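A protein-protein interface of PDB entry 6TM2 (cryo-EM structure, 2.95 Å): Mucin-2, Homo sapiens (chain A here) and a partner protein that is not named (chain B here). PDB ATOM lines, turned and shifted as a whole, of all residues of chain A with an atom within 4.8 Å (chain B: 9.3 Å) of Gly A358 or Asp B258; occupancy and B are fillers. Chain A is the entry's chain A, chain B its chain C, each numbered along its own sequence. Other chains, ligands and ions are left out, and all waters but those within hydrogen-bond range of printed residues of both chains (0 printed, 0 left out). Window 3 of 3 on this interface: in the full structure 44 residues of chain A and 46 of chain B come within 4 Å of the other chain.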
ATOM      1  N   CYS A 292       3.764  11.453  -0.924  1.00  0.00           N
ATOM      2  CA  CYS A 292       4.532  10.735  -1.959  1.00  0.00           C
ATOM      3  C   CYS A 292       5.637   9.804  -1.434  1.00  0.00           C
ATOM      4  O   CYS A 292       6.161   8.976  -2.183  1.00  0.00           O
ATOM      5  CB  CYS A 292       5.096  11.770  -2.954  1.00  0.00           C
ATOM      6  SG  CYS A 292       6.192  11.316  -4.315  1.00  0.00           S
ATOM      7  N   CYS A 331       6.362  10.169  -8.829  1.00  0.00           N
ATOM      8  CA  CYS A 331       7.175  10.153  -7.617  1.00  0.00           C
ATOM      9  C   CYS A 331       8.538   9.533  -7.884  1.00  0.00           C
ATOM     10  O   CYS A 331       8.648   8.335  -8.161  1.00  0.00           O
ATOM     11  CB  CYS A 331       6.449   9.401  -6.508  1.00  0.00           C
ATOM     12  SG  CYS A 331       5.113  10.305  -5.707  1.00  0.00           S
ATOM     13  N   CYS A 333      11.931   7.968  -6.781  1.00  0.00           N
ATOM     14  CA  CYS A 333      12.360   7.196  -5.629  1.00  0.00           C
ATOM     15  C   CYS A 333      13.669   7.762  -5.097  1.00  0.00           C
ATOM     16  O   CYS A 333      14.238   8.702  -5.654  1.00  0.00           O
ATOM     17  CB  CYS A 333      12.523   5.730  -6.009  1.00  0.00           C
ATOM     18  SG  CYS A 333      11.030   4.890  -6.553  1.00  0.00           S
ATOM     19  N   ARG A 334      14.169   7.187  -4.008  1.00  0.00           N
ATOM     20  CA  ARG A 334      15.503   7.537  -3.553  1.00  0.00           C
ATOM     21  C   ARG A 334      16.124   6.324  -2.885  1.00  0.00           C
ATOM     22  O   ARG A 334      15.425   5.442  -2.382  1.00  0.00           O
ATOM     23  CB  ARG A 334      15.507   8.735  -2.595  1.00  0.00           C
ATOM     24  CG  ARG A 334      14.960   8.479  -1.211  1.00  0.00           C
ATOM     25  CD  ARG A 334      14.951   9.767  -0.393  1.00  0.00           C
ATOM     26  NE  ARG A 334      14.623   9.540   1.015  1.00  0.00           N
ATOM     27  CZ  ARG A 334      13.395   9.523   1.524  1.00  0.00           C
ATOM     28  NH1 ARG A 334      12.339   9.723   0.746  1.00  0.00           N
ATOM     29  NH2 ARG A 334      13.225   9.307   2.817  1.00  0.00           N
ATOM     30  N   ASN A 356       8.879   2.075  -9.042  1.00  0.00           N
ATOM     31  CA  ASN A 356       7.486   2.236  -9.425  1.00  0.00           C
ATOM     32  C   ASN A 356       7.020   3.574  -8.837  1.00  0.00           C
ATOM     33  O   ASN A 356       7.847   4.431  -8.520  1.00  0.00           O
ATOM     34  CB  ASN A 356       6.695   1.005  -8.973  1.00  0.00           C
ATOM     35  CG  ASN A 356       5.349   0.884  -9.653  1.00  0.00           C
ATOM     36  OD1 ASN A 356       4.978   1.725 -10.468  1.00  0.00           O
ATOM     37  ND2 ASN A 356       4.606  -0.159  -9.312  1.00  0.00           N
ATOM     38  N   ALA A 357       5.712   3.801  -8.711  1.00  0.00           N
ATOM     39  CA  ALA A 357       5.186   5.092  -8.268  1.00  0.00           C
ATOM     40  C   ALA A 357       5.470   5.282  -6.781  1.00  0.00           C
ATOM     41  O   ALA A 357       4.622   5.060  -5.916  1.00  0.00           O
ATOM     42  CB  ALA A 357       3.695   5.181  -8.556  1.00  0.00           C
ATOM     43  N   GLY A 358       6.697   5.712  -6.485  1.00  0.00           N
ATOM     44  CA  GLY A 358       7.117   6.010  -5.139  1.00  0.00           C
ATOM     45  C   GLY A 358       7.733   4.853  -4.385  1.00  0.00           C
ATOM     46  O   GLY A 358       8.528   5.084  -3.471  1.00  0.00           O
ATOM     47  N   ARG A 359       7.393   3.619  -4.740  1.00  0.00           N
ATOM     48  CA  ARG A 359       7.886   2.436  -4.061  1.00  0.00           C
ATOM     49  C   ARG A 359       8.717   1.596  -5.018  1.00  0.00           C
ATOM     50  O   ARG A 359       8.601   1.709  -6.239  1.00  0.00           O
ATOM     51  CB  ARG A 359       6.732   1.603  -3.502  1.00  0.00           C
ATOM     52  CG  ARG A 359       5.804   1.073  -4.575  1.00  0.00           C
ATOM     53  CD  ARG A 359       4.683   0.243  -3.988  1.00  0.00           C
ATOM     54  NE  ARG A 359       5.181  -1.003  -3.419  1.00  0.00           N
ATOM     55  CZ  ARG A 359       5.364  -2.119  -4.113  1.00  0.00           C
ATOM     56  NH1 ARG A 359       5.074  -2.150  -5.402  1.00  0.00           N
ATOM     57  NH2 ARG A 359       5.829  -3.206  -3.520  1.00  0.00           N
ATOM     58  N   TRP A 360       9.565   0.749  -4.441  1.00  0.00           N
ATOM     59  CA  TRP A 360      10.418  -0.145  -5.207  1.00  0.00           C
ATOM     60  C   TRP A 360       9.740  -1.494  -5.388  1.00  0.00           C
ATOM     61  O   TRP A 360       9.087  -2.000  -4.475  1.00  0.00           O
ATOM     62  CB  TRP A 360      11.759  -0.345  -4.513  1.00  0.00           C
ATOM     63  CG  TRP A 360      12.624   0.851  -4.463  1.00  0.00           C
ATOM     64  CD1 TRP A 360      12.774   1.701  -3.420  1.00  0.00           C
ATOM     65  CD2 TRP A 360      13.487   1.330  -5.498  1.00  0.00           C
ATOM     66  NE1 TRP A 360      13.673   2.684  -3.733  1.00  0.00           N
ATOM     67  CE2 TRP A 360      14.125   2.478  -5.008  1.00  0.00           C
ATOM     68  CE3 TRP A 360      13.779   0.899  -6.794  1.00  0.00           C
ATOM     69  CZ2 TRP A 360      15.040   3.201  -5.765  1.00  0.00           C
ATOM     70  CZ3 TRP A 360      14.686   1.620  -7.542  1.00  0.00           C
ATOM     71  CH2 TRP A 360      15.304   2.757  -7.027  1.00  0.00           C
ATOM     72  N   CYS B 142       0.336  -1.367   4.895  1.00  0.00           N
ATOM     73  CA  CYS B 142       1.637  -1.684   4.317  1.00  0.00           C
ATOM     74  C   CYS B 142       1.453  -1.855   2.819  1.00  0.00           C
ATOM     75  O   CYS B 142       1.356  -2.976   2.322  1.00  0.00           O
ATOM     76  CB  CYS B 142       2.222  -2.952   4.956  1.00  0.00           C
ATOM     77  SG  CYS B 142       2.513  -2.866   6.743  1.00  0.00           S
ATOM     78  N   GLY B 143       1.421  -0.745   2.097  1.00  0.00           N
ATOM     79  CA  GLY B 143       1.270  -0.781   0.654  1.00  0.00           C
ATOM     80  C   GLY B 143      -0.116  -1.169   0.182  1.00  0.00           C
ATOM     81  O   GLY B 143      -0.310  -2.232  -0.407  1.00  0.00           O
ATOM     82  N   CYS B 240       4.033  -4.463   8.998  1.00  0.00           N
ATOM     83  CA  CYS B 240       5.334  -3.843   8.762  1.00  0.00           C
ATOM     84  C   CYS B 240       5.597  -2.844   9.880  1.00  0.00           C
ATOM     85  O   CYS B 240       4.777  -2.670  10.780  1.00  0.00           O
ATOM     86  CB  CYS B 240       5.414  -3.189   7.378  1.00  0.00           C
ATOM     87  SG  CYS B 240       4.255  -1.873   7.020  1.00  0.00           S
ATOM     88  N   PHE B 254      14.491  -5.938   7.679  1.00  0.00           N
ATOM     89  CA  PHE B 254      14.893  -4.565   7.398  1.00  0.00           C
ATOM     90  C   PHE B 254      14.364  -4.092   6.052  1.00  0.00           C
ATOM     91  O   PHE B 254      15.102  -3.617   5.209  1.00  0.00           O
ATOM     92  CB  PHE B 254      16.406  -4.402   7.470  1.00  0.00           C
ATOM     93  CG  PHE B 254      16.985  -4.482   8.860  1.00  0.00           C
ATOM     94  CD1 PHE B 254      16.176  -4.559   9.977  1.00  0.00           C
ATOM     95  CD2 PHE B 254      18.345  -4.370   9.048  1.00  0.00           C
ATOM     96  CE1 PHE B 254      16.708  -4.601  11.229  1.00  0.00           C
ATOM     97  CE2 PHE B 254      18.880  -4.405  10.313  1.00  0.00           C
ATOM     98  CZ  PHE B 254      18.057  -4.512  11.398  1.00  0.00           C
ATOM     99  N   THR B 255      13.057  -4.208   5.863  1.00  0.00           N
ATOM    100  CA  THR B 255      12.369  -3.620   4.726  1.00  0.00           C
ATOM    101  C   THR B 255      11.944  -2.209   5.099  1.00  0.00           C
ATOM    102  O   THR B 255      11.314  -2.005   6.137  1.00  0.00           O
ATOM    103  CB  THR B 255      11.146  -4.448   4.337  1.00  0.00           C
ATOM    104  OG1 THR B 255      11.549  -5.778   4.016  1.00  0.00           O
ATOM    105  CG2 THR B 255      10.484  -3.858   3.130  1.00  0.00           C
ATOM    106  N   THR B 256      12.283  -1.240   4.257  1.00  0.00           N
ATOM    107  CA  THR B 256      11.970   0.145   4.553  1.00  0.00           C
ATOM    108  C   THR B 256      10.531   0.453   4.145  1.00  0.00           C
ATOM    109  O   THR B 256       9.788  -0.419   3.698  1.00  0.00           O
ATOM    110  CB  THR B 256      12.970   1.064   3.864  1.00  0.00           C
ATOM    111  OG1 THR B 256      12.910   0.859   2.451  1.00  0.00           O
ATOM    112  CG2 THR B 256      14.369   0.768   4.333  1.00  0.00           C
ATOM    113  N   ARG B 257      10.121   1.712   4.330  1.00  0.00           N
ATOM    114  CA  ARG B 257       8.759   2.127   4.003  1.00  0.00           C
ATOM    115  C   ARG B 257       8.482   2.046   2.506  1.00  0.00           C
ATOM    116  O   ARG B 257       7.346   1.791   2.097  1.00  0.00           O
ATOM    117  CB  ARG B 257       8.506   3.541   4.531  1.00  0.00           C
ATOM    118  CG  ARG B 257       7.072   4.025   4.398  1.00  0.00           C
ATOM    119  CD  ARG B 257       6.860   5.460   4.839  1.00  0.00           C
ATOM    120  NE  ARG B 257       6.956   5.727   6.270  1.00  0.00           N
ATOM    121  CZ  ARG B 257       5.939   5.631   7.117  1.00  0.00           C
ATOM    122  NH1 ARG B 257       4.746   5.262   6.685  1.00  0.00           N
ATOM    123  NH2 ARG B 257       6.105   5.919   8.391  1.00  0.00           N
ATOM    124  N   ASP B 258       9.505   2.215   1.671  1.00  0.00           N
ATOM    125  CA  ASP B 258       9.359   2.094   0.226  1.00  0.00           C
ATOM    126  C   ASP B 258       9.684   0.699  -0.297  1.00  0.00           C
ATOM    127  O   ASP B 258      10.096   0.577  -1.453  1.00  0.00           O
ATOM    128  CB  ASP B 258      10.214   3.144  -0.477  1.00  0.00           C
ATOM    129  CG  ASP B 258      11.682   3.053  -0.118  1.00  0.00           C
ATOM    130  OD1 ASP B 258      12.061   2.245   0.755  1.00  0.00           O
ATOM    131  OD2 ASP B 258      12.473   3.802  -0.727  1.00  0.00           O
ATOM    132  N   HIS B 259       9.543  -0.332   0.547  1.00  0.00           N
ATOM    133  CA  HIS B 259       9.591  -1.749   0.170  1.00  0.00           C
ATOM    134  C   HIS B 259      10.955  -2.162  -0.377  1.00  0.00           C
ATOM    135  O   HIS B 259      11.065  -2.822  -1.407  1.00  0.00           O
ATOM    136  CB  HIS B 259       8.482  -2.090  -0.822  1.00  0.00           C
ATOM    137  CG  HIS B 259       7.107  -1.939  -0.263  1.00  0.00           C
ATOM    138  ND1 HIS B 259       6.541  -2.868   0.576  1.00  0.00           N
ATOM    139  CD2 HIS B 259       6.183  -0.964  -0.423  1.00  0.00           C
ATOM    140  CE1 HIS B 259       5.322  -2.478   0.901  1.00  0.00           C
ATOM    141  NE2 HIS B 259       5.082  -1.324   0.307  1.00  0.00           N
ATOM    142  N   MET B 260      12.002  -1.782   0.341  1.00  0.00           N
ATOM    143  CA  MET B 260      13.380  -2.064  -0.029  1.00  0.00           C
ATOM    144  C   MET B 260      14.107  -2.658   1.161  1.00  0.00           C
ATOM    145  O   MET B 260      14.130  -2.057   2.235  1.00  0.00           O
ATOM    146  CB  MET B 260      14.076  -0.789  -0.495  1.00  0.00           C
ATOM    147  CG  MET B 260      15.525  -0.946  -0.882  1.00  0.00           C
ATOM    148  SD  MET B 260      15.877  -1.964  -2.311  1.00  0.00           S
ATOM    149  CE  MET B 260      17.545  -2.455  -1.894  1.00  0.00           C
ATOM    150  N   VAL B 261      14.703  -3.829   0.976  1.00  0.00           N
ATOM    151  CA  VAL B 261      15.449  -4.488   2.039  1.00  0.00           C
ATOM    152  C   VAL B 261      16.861  -3.922   2.043  1.00  0.00           C
ATOM    153  O   VAL B 261      17.629  -4.133   1.104  1.00  0.00           O
ATOM    154  CB  VAL B 261      15.461  -6.010   1.871  1.00  0.00           C
ATOM    155  CG1 VAL B 261      16.302  -6.630   2.942  1.00  0.00           C
ATOM    156  CG2 VAL B 261      14.071  -6.550   1.967  1.00  0.00           C
ATOM    157  N   VAL B 262      17.204  -3.201   3.104  1.00  0.00           N
ATOM    158  CA  VAL B 262      18.528  -2.630   3.276  1.00  0.00           C
ATOM    159  C   VAL B 262      19.270  -3.441   4.331  1.00  0.00           C
ATOM    160  O   VAL B 262      18.697  -4.289   5.009  1.00  0.00           O
ATOM    161  CB  VAL B 262      18.466  -1.139   3.652  1.00  0.00           C
ATOM    162  CG1 VAL B 262      17.828  -0.349   2.534  1.00  0.00           C
ATOM    163  CG2 VAL B 262      17.690  -0.944   4.922  1.00  0.00           C
ATOM    164  N   ASP B 267      19.330   3.106   8.059  1.00  0.00           N
ATOM    165  CA  ASP B 267      18.505   3.420   6.901  1.00  0.00           C
ATOM    166  C   ASP B 267      17.116   2.838   7.025  1.00  0.00           C
ATOM    167  O   ASP B 267      16.168   3.402   6.478  1.00  0.00           O
ATOM    168  CB  ASP B 267      19.139   2.885   5.620  1.00  0.00           C
ATOM    169  CG  ASP B 267      20.382   3.632   5.223  1.00  0.00           C
ATOM    170  OD1 ASP B 267      20.494   4.834   5.531  1.00  0.00           O
ATOM    171  OD2 ASP B 267      21.248   3.012   4.584  1.00  0.00           O
ATOM    172  N   PHE B 268      16.999   1.701   7.707  1.00  0.00           N
ATOM    173  CA  PHE B 268      15.708   1.094   8.013  1.00  0.00           C
ATOM    174  C   PHE B 268      14.937   1.888   9.054  1.00  0.00           C
ATOM    175  O   PHE B 268      13.776   2.240   8.832  1.00  0.00           O
ATOM    176  CB  PHE B 268      15.941  -0.350   8.454  1.00  0.00           C
ATOM    177  CG  PHE B 268      14.764  -1.011   9.097  1.00  0.00           C
ATOM    178  CD1 PHE B 268      13.634  -1.331   8.393  1.00  0.00           C
ATOM    179  CD2 PHE B 268      14.842  -1.392  10.423  1.00  0.00           C
ATOM    180  CE1 PHE B 268      12.586  -1.957   9.019  1.00  0.00           C
ATOM    181  CE2 PHE B 268      13.798  -2.023  11.035  1.00  0.00           C
ATOM    182  CZ  PHE B 268      12.676  -2.304  10.336  1.00  0.00           C
ATOM    183  N   ASN B 270      15.336   4.987  10.146  1.00  0.00           N
ATOM    184  CA  ASN B 270      15.038   6.359   9.758  1.00  0.00           C
ATOM    185  C   ASN B 270      13.929   6.469   8.729  1.00  0.00           C
ATOM    186  O   ASN B 270      13.505   7.583   8.424  1.00  0.00           O
ATOM    187  CB  ASN B 270      16.278   7.057   9.202  1.00  0.00           C
ATOM    188  CG  ASN B 270      17.272   7.438  10.272  1.00  0.00           C
ATOM    189  OD1 ASN B 270      16.900   7.901  11.343  1.00  0.00           O
ATOM    190  ND2 ASN B 270      18.546   7.270   9.975  1.00  0.00           N
ATOM    191  N   SER B 271      13.450   5.366   8.181  1.00  0.00           N
ATOM    192  CA  SER B 271      12.376   5.410   7.209  1.00  0.00           C
ATOM    193  C   SER B 271      11.008   5.201   7.826  1.00  0.00           C
ATOM    194  O   SER B 271      10.007   5.331   7.126  1.00  0.00           O
ATOM    195  CB  SER B 271      12.612   4.373   6.120  1.00  0.00           C
ATOM    196  OG  SER B 271      12.581   3.078   6.656  1.00  0.00           O
ATOM    197  N   TRP B 272      10.934   4.882   9.114  1.00  0.00           N
ATOM    198  CA  TRP B 272       9.654   4.685   9.770  1.00  0.00           C
ATOM    199  C   TRP B 272       9.304   5.824  10.708  1.00  0.00           C
ATOM    200  O   TRP B 272       8.380   5.683  11.504  1.00  0.00           O
ATOM    201  CB  TRP B 272       9.611   3.350  10.517  1.00  0.00           C
ATOM    202  CG  TRP B 272       9.622   2.185   9.601  1.00  0.00           C
ATOM    203  CD1 TRP B 272      10.663   1.357   9.337  1.00  0.00           C
ATOM    204  CD2 TRP B 272       8.561   1.776   8.749  1.00  0.00           C
ATOM    205  NE1 TRP B 272      10.302   0.430   8.408  1.00  0.00           N
ATOM    206  CE2 TRP B 272       9.014   0.675   8.021  1.00  0.00           C
ATOM    207  CE3 TRP B 272       7.263   2.231   8.537  1.00  0.00           C
ATOM    208  CZ2 TRP B 272       8.215   0.017   7.107  1.00  0.00           C
ATOM    209  CZ3 TRP B 272       6.474   1.582   7.632  1.00  0.00           C
ATOM    210  CH2 TRP B 272       6.948   0.491   6.926  1.00  0.00           C
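N of Trp A360 sits at hydrogen-bond distance from O of Asp B258 (3.0 Å).
SG of Cys A331 forms a disulfide with SG of Cys A292, 2.0 Å away.
The side-chain sulfur (SG) of Cys B240 is disulfide-bonded to the side-chain sulfur (SG) of Cys B142 (2.0 Å).
OD2 of Asp B258 touches O of Arg A334 (3.8 Å).
Gly A358 touches Asp B258.
Asp B258 touches Arg A359 (O to CA, 3.9 Å).
Arg A359 touches His B259 (NE to CD2, 3.2 Å).
Trp A360 touches His B259.
No residue of chain B comes within 4 Å of Cys A331.
Of the printed residues of chain B, Arg A334 touches Asp B258.
No residue of chain B comes within 4 Å of Ala A357.
Gly A358 touches just one residue of chain B: Asp B258.
Of the printed residues of chain B, Arg A359 touches Asp B258 (3.9 Å) and His B259 (3.2 Å).
Cys B240 touches none of the printed residues of chain A.
Thr B256 touches none of the printed residues of chain A.
Asp B258 touches just these residues of chain A: Arg A334 (3.8 Å), Gly A358 (3.9 Å), Arg A359 (3.9 Å) and Trp A360 (3.0 Å).
Printed residues of chain A within 4 Å of His B259: Arg A359 and Trp A360.
The nearest residue of chain B that does not touch Gly A358 is Arg B257 (6.6 Å).
The nearest printed residue of chain A that does not touch Asp B258 is Cys A333 (5.6 Å).
Of the 17 printed residues of chain B, 2 touch a printed residue of chain A.
Among the printed residues, 6 pairs touch across the chains.
Among the printed residues, no Asp or Glu carboxylate lies within 4 Å of a Lys or Arg side-chain nitrogen of the other chain.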
